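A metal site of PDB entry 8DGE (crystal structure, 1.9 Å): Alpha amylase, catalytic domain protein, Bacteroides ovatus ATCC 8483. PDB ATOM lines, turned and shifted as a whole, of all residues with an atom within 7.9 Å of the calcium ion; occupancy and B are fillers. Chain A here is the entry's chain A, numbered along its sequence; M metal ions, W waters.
The calcium ion is bound by O of Phe 337, at 2.2 Å. OD2 of Asp 354 binds the calcium ion, 2.3 Å away. OE1 of Glu 254 binds the calcium ion (2.4 Å). The calcium ion is bound by water W1, 2.4 Å away. O of Gly 339 is bound to the calcium ion, at 2.4 Å. The calcium ion is bound by OE1 of Glu 336 (2.5 Å). The side-chain carboxylate (OE2) of Glu 336 is bound to the calcium ion, 2.8 Å away.
The side-chain carboxylate of Asp 354 is in hydrogen-bond range of the side-chain hydroxyl of Ser 356, 2.7 Å away. The backbone NH (N) of Glu 254 lies within hydrogen-bond range of the side-chain carboxylate (OD2) of Asp 258. The side-chain carboxylate (OE1) of Glu 336 sits close to the side-chain hydroxyl (OH) of Tyr 269, 2.6 Å away. N of Gly 348 sits at hydrogen-bond distance from O of Glu 336 (2.8 Å). The backbone carbonyl oxygen (O) of Val 334 lies within hydrogen-bond range of the backbone NH (N) of Asp 354, at 2.7 Å.
The nearest printed residue that does not touch the calcium ion is Ala 338 (4.3 Å).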
ATOM      1  N   ALA A 252      31.237  24.778   4.532  1.00  0.00           N
ATOM      2  CA  ALA A 252      32.373  25.153   5.391  1.00  0.00           C
ATOM      3  C   ALA A 252      32.244  24.449   6.739  1.00  0.00           C
ATOM      4  O   ALA A 252      31.110  24.248   7.212  1.00  0.00           O
ATOM      5  CB  ALA A 252      32.389  26.654   5.549  1.00  0.00           C
ATOM      6  N   LEU A 253      33.367  24.068   7.335  1.00  0.00           N
ATOM      7  CA  LEU A 253      33.417  23.726   8.773  1.00  0.00           C
ATOM      8  C   LEU A 253      34.010  24.935   9.494  1.00  0.00           C
ATOM      9  O   LEU A 253      34.925  25.593   8.937  1.00  0.00           O
ATOM     10  CB  LEU A 253      34.204  22.430   8.981  1.00  0.00           C
ATOM     11  CG  LEU A 253      33.676  21.213   8.214  1.00  0.00           C
ATOM     12  CD1 LEU A 253      34.551  19.986   8.442  1.00  0.00           C
ATOM     13  CD2 LEU A 253      32.241  20.905   8.589  1.00  0.00           C
ATOM     14  N   GLU A 254      33.436  25.284  10.644  1.00  0.00           N
ATOM     15  CA  GLU A 254      33.849  26.431  11.490  1.00  0.00           C
ATOM     16  C   GLU A 254      34.419  25.877  12.809  1.00  0.00           C
ATOM     17  O   GLU A 254      33.750  25.046  13.454  1.00  0.00           O
ATOM     18  CB  GLU A 254      32.641  27.336  11.735  1.00  0.00           C
ATOM     19  CG  GLU A 254      32.996  28.643  12.418  1.00  0.00           C
ATOM     20  CD  GLU A 254      31.800  29.540  12.689  1.00  0.00           C
ATOM     21  OE1 GLU A 254      30.670  29.173  12.292  1.00  0.00           O
ATOM     22  OE2 GLU A 254      32.005  30.606  13.308  1.00  0.00           O
ATOM     23  N   VAL A 257      32.456  25.345  16.458  1.00  0.00           N
ATOM     24  CA  VAL A 257      31.062  24.877  16.171  1.00  0.00           C
ATOM     25  C   VAL A 257      31.106  23.411  15.707  1.00  0.00           C
ATOM     26  O   VAL A 257      30.515  22.553  16.398  1.00  0.00           O
ATOM     27  CB  VAL A 257      30.367  25.759  15.112  1.00  0.00           C
ATOM     28  CG1 VAL A 257      28.975  25.249  14.761  1.00  0.00           C
ATOM     29  CG2 VAL A 257      30.313  27.219  15.534  1.00  0.00           C
ATOM     30  N   ASP A 258      31.767  23.132  14.576  1.00  0.00           N
ATOM     31  CA  ASP A 258      31.846  21.782  13.971  1.00  0.00           C
ATOM     32  C   ASP A 258      32.878  20.964  14.757  1.00  0.00           C
ATOM     33  O   ASP A 258      34.031  21.413  14.849  1.00  0.00           O
ATOM     34  CB  ASP A 258      32.147  21.879  12.473  1.00  0.00           C
ATOM     35  CG  ASP A 258      31.035  22.557  11.683  1.00  0.00           C
ATOM     36  OD1 ASP A 258      29.961  21.929  11.522  1.00  0.00           O
ATOM     37  OD2 ASP A 258      31.233  23.699  11.255  1.00  0.00           O
ATOM     38  N   TYR A 269      37.775  28.901   9.317  1.00  0.00           N
ATOM     39  CA  TYR A 269      37.034  28.149   8.256  1.00  0.00           C
ATOM     40  C   TYR A 269      37.943  27.227   7.433  1.00  0.00           C
ATOM     41  O   TYR A 269      39.028  27.645   6.977  1.00  0.00           O
ATOM     42  CB  TYR A 269      36.351  29.112   7.268  1.00  0.00           C
ATOM     43  CG  TYR A 269      35.085  29.804   7.730  1.00  0.00           C
ATOM     44  CD1 TYR A 269      34.041  29.101   8.316  1.00  0.00           C
ATOM     45  CD2 TYR A 269      34.919  31.170   7.541  1.00  0.00           C
ATOM     46  CE1 TYR A 269      32.878  29.737   8.721  1.00  0.00           C
ATOM     47  CE2 TYR A 269      33.759  31.824   7.943  1.00  0.00           C
ATOM     48  CZ  TYR A 269      32.733  31.109   8.536  1.00  0.00           C
ATOM     49  OH  TYR A 269      31.582  31.741   8.935  1.00  0.00           O
ATOM     50  N   VAL A 334      20.661  33.475   6.609  1.00  0.00           N
ATOM     51  CA  VAL A 334      20.991  32.018   6.658  1.00  0.00           C
ATOM     52  C   VAL A 334      22.399  31.766   6.082  1.00  0.00           C
ATOM     53  O   VAL A 334      22.875  30.634   6.209  1.00  0.00           O
ATOM     54  CB  VAL A 334      19.937  31.163   5.915  1.00  0.00           C
ATOM     55  CG1 VAL A 334      18.620  31.129   6.666  1.00  0.00           C
ATOM     56  CG2 VAL A 334      19.746  31.633   4.479  1.00  0.00           C
ATOM     57  N   GLN A 335      23.037  32.773   5.478  1.00  0.00           N
ATOM     58  CA  GLN A 335      24.446  32.659   5.001  1.00  0.00           C
ATOM     59  C   GLN A 335      25.371  32.510   6.215  1.00  0.00           C
ATOM     60  O   GLN A 335      25.059  33.116   7.266  1.00  0.00           O
ATOM     61  CB  GLN A 335      24.818  33.856   4.133  1.00  0.00           C
ATOM     62  CG  GLN A 335      24.160  33.792   2.767  1.00  0.00           C
ATOM     63  CD  GLN A 335      24.025  35.155   2.135  1.00  0.00           C
ATOM     64  OE1 GLN A 335      23.456  36.062   2.712  1.00  0.00           O
ATOM     65  NE2 GLN A 335      24.560  35.299   0.940  1.00  0.00           N
ATOM     66  N   GLU A 336      26.440  31.715   6.070  1.00  0.00           N
ATOM     67  CA  GLU A 336      27.382  31.338   7.155  1.00  0.00           C
ATOM     68  C   GLU A 336      27.702  32.573   8.002  1.00  0.00           C
ATOM     69  O   GLU A 336      28.287  33.525   7.448  1.00  0.00           O
ATOM     70  CB  GLU A 336      28.694  30.760   6.620  1.00  0.00           C
ATOM     71  CG  GLU A 336      29.057  29.409   7.192  1.00  0.00           C
ATOM     72  CD  GLU A 336      29.092  29.265   8.702  1.00  0.00           C
ATOM     73  OE1 GLU A 336      29.492  30.216   9.394  1.00  0.00           O
ATOM     74  OE2 GLU A 336      28.699  28.186   9.184  1.00  0.00           O
ATOM     75  N   PHE A 337      27.298  32.551   9.269  1.00  0.00           N
ATOM     76  CA  PHE A 337      27.562  33.641  10.245  1.00  0.00           C
ATOM     77  C   PHE A 337      28.451  33.093  11.362  1.00  0.00           C
ATOM     78  O   PHE A 337      28.528  31.856  11.554  1.00  0.00           O
ATOM     79  CB  PHE A 337      26.248  34.237  10.756  1.00  0.00           C
ATOM     80  CG  PHE A 337      25.272  33.227  11.295  1.00  0.00           C
ATOM     81  CD1 PHE A 337      25.460  32.659  12.550  1.00  0.00           C
ATOM     82  CD2 PHE A 337      24.176  32.819  10.536  1.00  0.00           C
ATOM     83  CE1 PHE A 337      24.561  31.719  13.031  1.00  0.00           C
ATOM     84  CE2 PHE A 337      23.274  31.893  11.035  1.00  0.00           C
ATOM     85  CZ  PHE A 337      23.480  31.339  12.271  1.00  0.00           C
ATOM     86  N   ALA A 338      29.148  33.992  12.056  1.00  0.00           N
ATOM     87  CA  ALA A 338      30.051  33.659  13.186  1.00  0.00           C
ATOM     88  C   ALA A 338      29.272  32.847  14.230  1.00  0.00           C
ATOM     89  O   ALA A 338      28.180  33.300  14.668  1.00  0.00           O
ATOM     90  CB  ALA A 338      30.623  34.925  13.786  1.00  0.00           C
ATOM     91  N   GLY A 339      29.824  31.688  14.592  1.00  0.00           N
ATOM     92  CA  GLY A 339      29.253  30.760  15.587  1.00  0.00           C
ATOM     93  C   GLY A 339      27.958  30.141  15.103  1.00  0.00           C
ATOM     94  O   GLY A 339      27.780  30.034  13.869  1.00  0.00           O
ATOM     95  N   ASN A 340      27.080  29.759  16.026  1.00  0.00           N
ATOM     96  CA  ASN A 340      25.845  29.002  15.711  1.00  0.00           C
ATOM     97  C   ASN A 340      24.657  29.502  16.547  1.00  0.00           C
ATOM     98  O   ASN A 340      23.687  28.729  16.692  1.00  0.00           O
ATOM     99  CB  ASN A 340      26.074  27.504  15.910  1.00  0.00           C
ATOM    100  CG  ASN A 340      26.372  27.129  17.345  1.00  0.00           C
ATOM    101  OD1 ASN A 340      26.519  27.988  18.221  1.00  0.00           O
ATOM    102  ND2 ASN A 340      26.467  25.836  17.595  1.00  0.00           N
ATOM    103  N   ASP A 341      24.714  30.732  17.063  1.00  0.00           N
ATOM    104  CA  ASP A 341      23.642  31.337  17.908  1.00  0.00           C
ATOM    105  C   ASP A 341      23.598  32.845  17.649  1.00  0.00           C
ATOM    106  O   ASP A 341      24.295  33.596  18.383  1.00  0.00           O
ATOM    107  CB  ASP A 341      23.849  31.016  19.392  1.00  0.00           C
ATOM    108  CG  ASP A 341      22.904  31.746  20.328  1.00  0.00           C
ATOM    109  OD1 ASP A 341      21.999  32.452  19.818  1.00  0.00           O
ATOM    110  OD2 ASP A 341      23.090  31.634  21.545  1.00  0.00           O
ATOM    111  N   SER A 342      22.800  33.264  16.666  1.00  0.00           N
ATOM    112  CA  SER A 342      22.837  34.611  16.050  1.00  0.00           C
ATOM    113  C   SER A 342      21.508  34.907  15.333  1.00  0.00           C
ATOM    114  O   SER A 342      20.865  33.968  14.839  1.00  0.00           O
ATOM    115  CB  SER A 342      23.993  34.712  15.087  1.00  0.00           C
ATOM    116  OG  SER A 342      24.164  36.037  14.615  1.00  0.00           O
ATOM    117  N   ASN A 346      25.989  38.884  10.638  1.00  0.00           N
ATOM    118  CA  ASN A 346      27.416  38.737  10.971  1.00  0.00           C
ATOM    119  C   ASN A 346      27.959  37.629  10.059  1.00  0.00           C
ATOM    120  O   ASN A 346      28.427  36.597  10.553  1.00  0.00           O
ATOM    121  CB  ASN A 346      27.582  38.539  12.473  1.00  0.00           C
ATOM    122  CG  ASN A 346      29.035  38.556  12.896  1.00  0.00           C
ATOM    123  OD1 ASN A 346      29.886  38.954  12.111  1.00  0.00           O
ATOM    124  ND2 ASN A 346      29.324  38.141  14.126  1.00  0.00           N
ATOM    125  N   GLY A 348      30.186  35.568   7.530  1.00  0.00           N
ATOM    126  CA  GLY A 348      31.601  35.271   7.207  1.00  0.00           C
ATOM    127  C   GLY A 348      31.771  34.727   5.802  1.00  0.00           C
ATOM    128  O   GLY A 348      32.826  34.983   5.192  1.00  0.00           O
ATOM    129  N   LEU A 353      25.707  28.481   3.170  1.00  0.00           N
ATOM    130  CA  LEU A 353      24.616  28.712   4.169  1.00  0.00           C
ATOM    131  C   LEU A 353      25.014  28.012   5.472  1.00  0.00           C
ATOM    132  O   LEU A 353      25.842  27.077   5.409  1.00  0.00           O
ATOM    133  CB  LEU A 353      23.290  28.191   3.616  1.00  0.00           C
ATOM    134  CG  LEU A 353      22.452  29.190   2.822  1.00  0.00           C
ATOM    135  CD1 LEU A 353      23.314  30.123   1.986  1.00  0.00           C
ATOM    136  CD2 LEU A 353      21.443  28.472   1.948  1.00  0.00           C
ATOM    137  N   ASP A 354      24.505  28.490   6.603  1.00  0.00           N
ATOM    138  CA  ASP A 354      24.957  28.064   7.950  1.00  0.00           C
ATOM    139  C   ASP A 354      24.403  26.669   8.264  1.00  0.00           C
ATOM    140  O   ASP A 354      23.171  26.514   8.325  1.00  0.00           O
ATOM    141  CB  ASP A 354      24.597  29.094   9.030  1.00  0.00           C
ATOM    142  CG  ASP A 354      25.446  28.890  10.267  1.00  0.00           C
ATOM    143  OD1 ASP A 354      25.258  27.855  10.930  1.00  0.00           O
ATOM    144  OD2 ASP A 354      26.347  29.724  10.502  1.00  0.00           O
ATOM    145  N   ALA A 355      25.316  25.711   8.479  1.00  0.00           N
ATOM    146  CA  ALA A 355      25.055  24.284   8.780  1.00  0.00           C
ATOM    147  C   ALA A 355      24.290  24.107  10.101  1.00  0.00           C
ATOM    148  O   ALA A 355      23.771  22.987  10.306  1.00  0.00           O
ATOM    149  CB  ALA A 355      26.374  23.534   8.806  1.00  0.00           C
ATOM    150  N   SER A 356      24.211  25.126  10.961  1.00  0.00           N
ATOM    151  CA  SER A 356      23.484  25.033  12.265  1.00  0.00           C
ATOM    152  C   SER A 356      21.968  24.899  12.006  1.00  0.00           C
ATOM    153  O   SER A 356      21.290  24.330  12.881  1.00  0.00           O
ATOM    154  CB  SER A 356      23.787  26.198  13.173  1.00  0.00           C
ATOM    155  OG  SER A 356      23.263  27.424  12.668  1.00  0.00           O
ATOM    156  N   ASP A 389      36.433  36.718   9.751  1.00  0.00           N
ATOM    157  CA  ASP A 389      36.551  35.327   9.248  1.00  0.00           C
ATOM    158  C   ASP A 389      36.540  35.288   7.718  1.00  0.00           C
ATOM    159  O   ASP A 389      37.009  34.276   7.146  1.00  0.00           O
ATOM    160  CB  ASP A 389      35.422  34.436   9.787  1.00  0.00           C
ATOM    161  CG  ASP A 389      35.411  34.249  11.293  1.00  0.00           C
ATOM    162  OD1 ASP A 389      36.441  34.570  11.947  1.00  0.00           O
ATOM    163  OD2 ASP A 389      34.374  33.781  11.814  1.00  0.00           O
HETATM  164 CA    CA M   1      28.435  29.624  11.553  1.00  0.00          CA
HETATM  165  O   HOH W   1      27.703  27.369  11.950  1.00  0.00           O
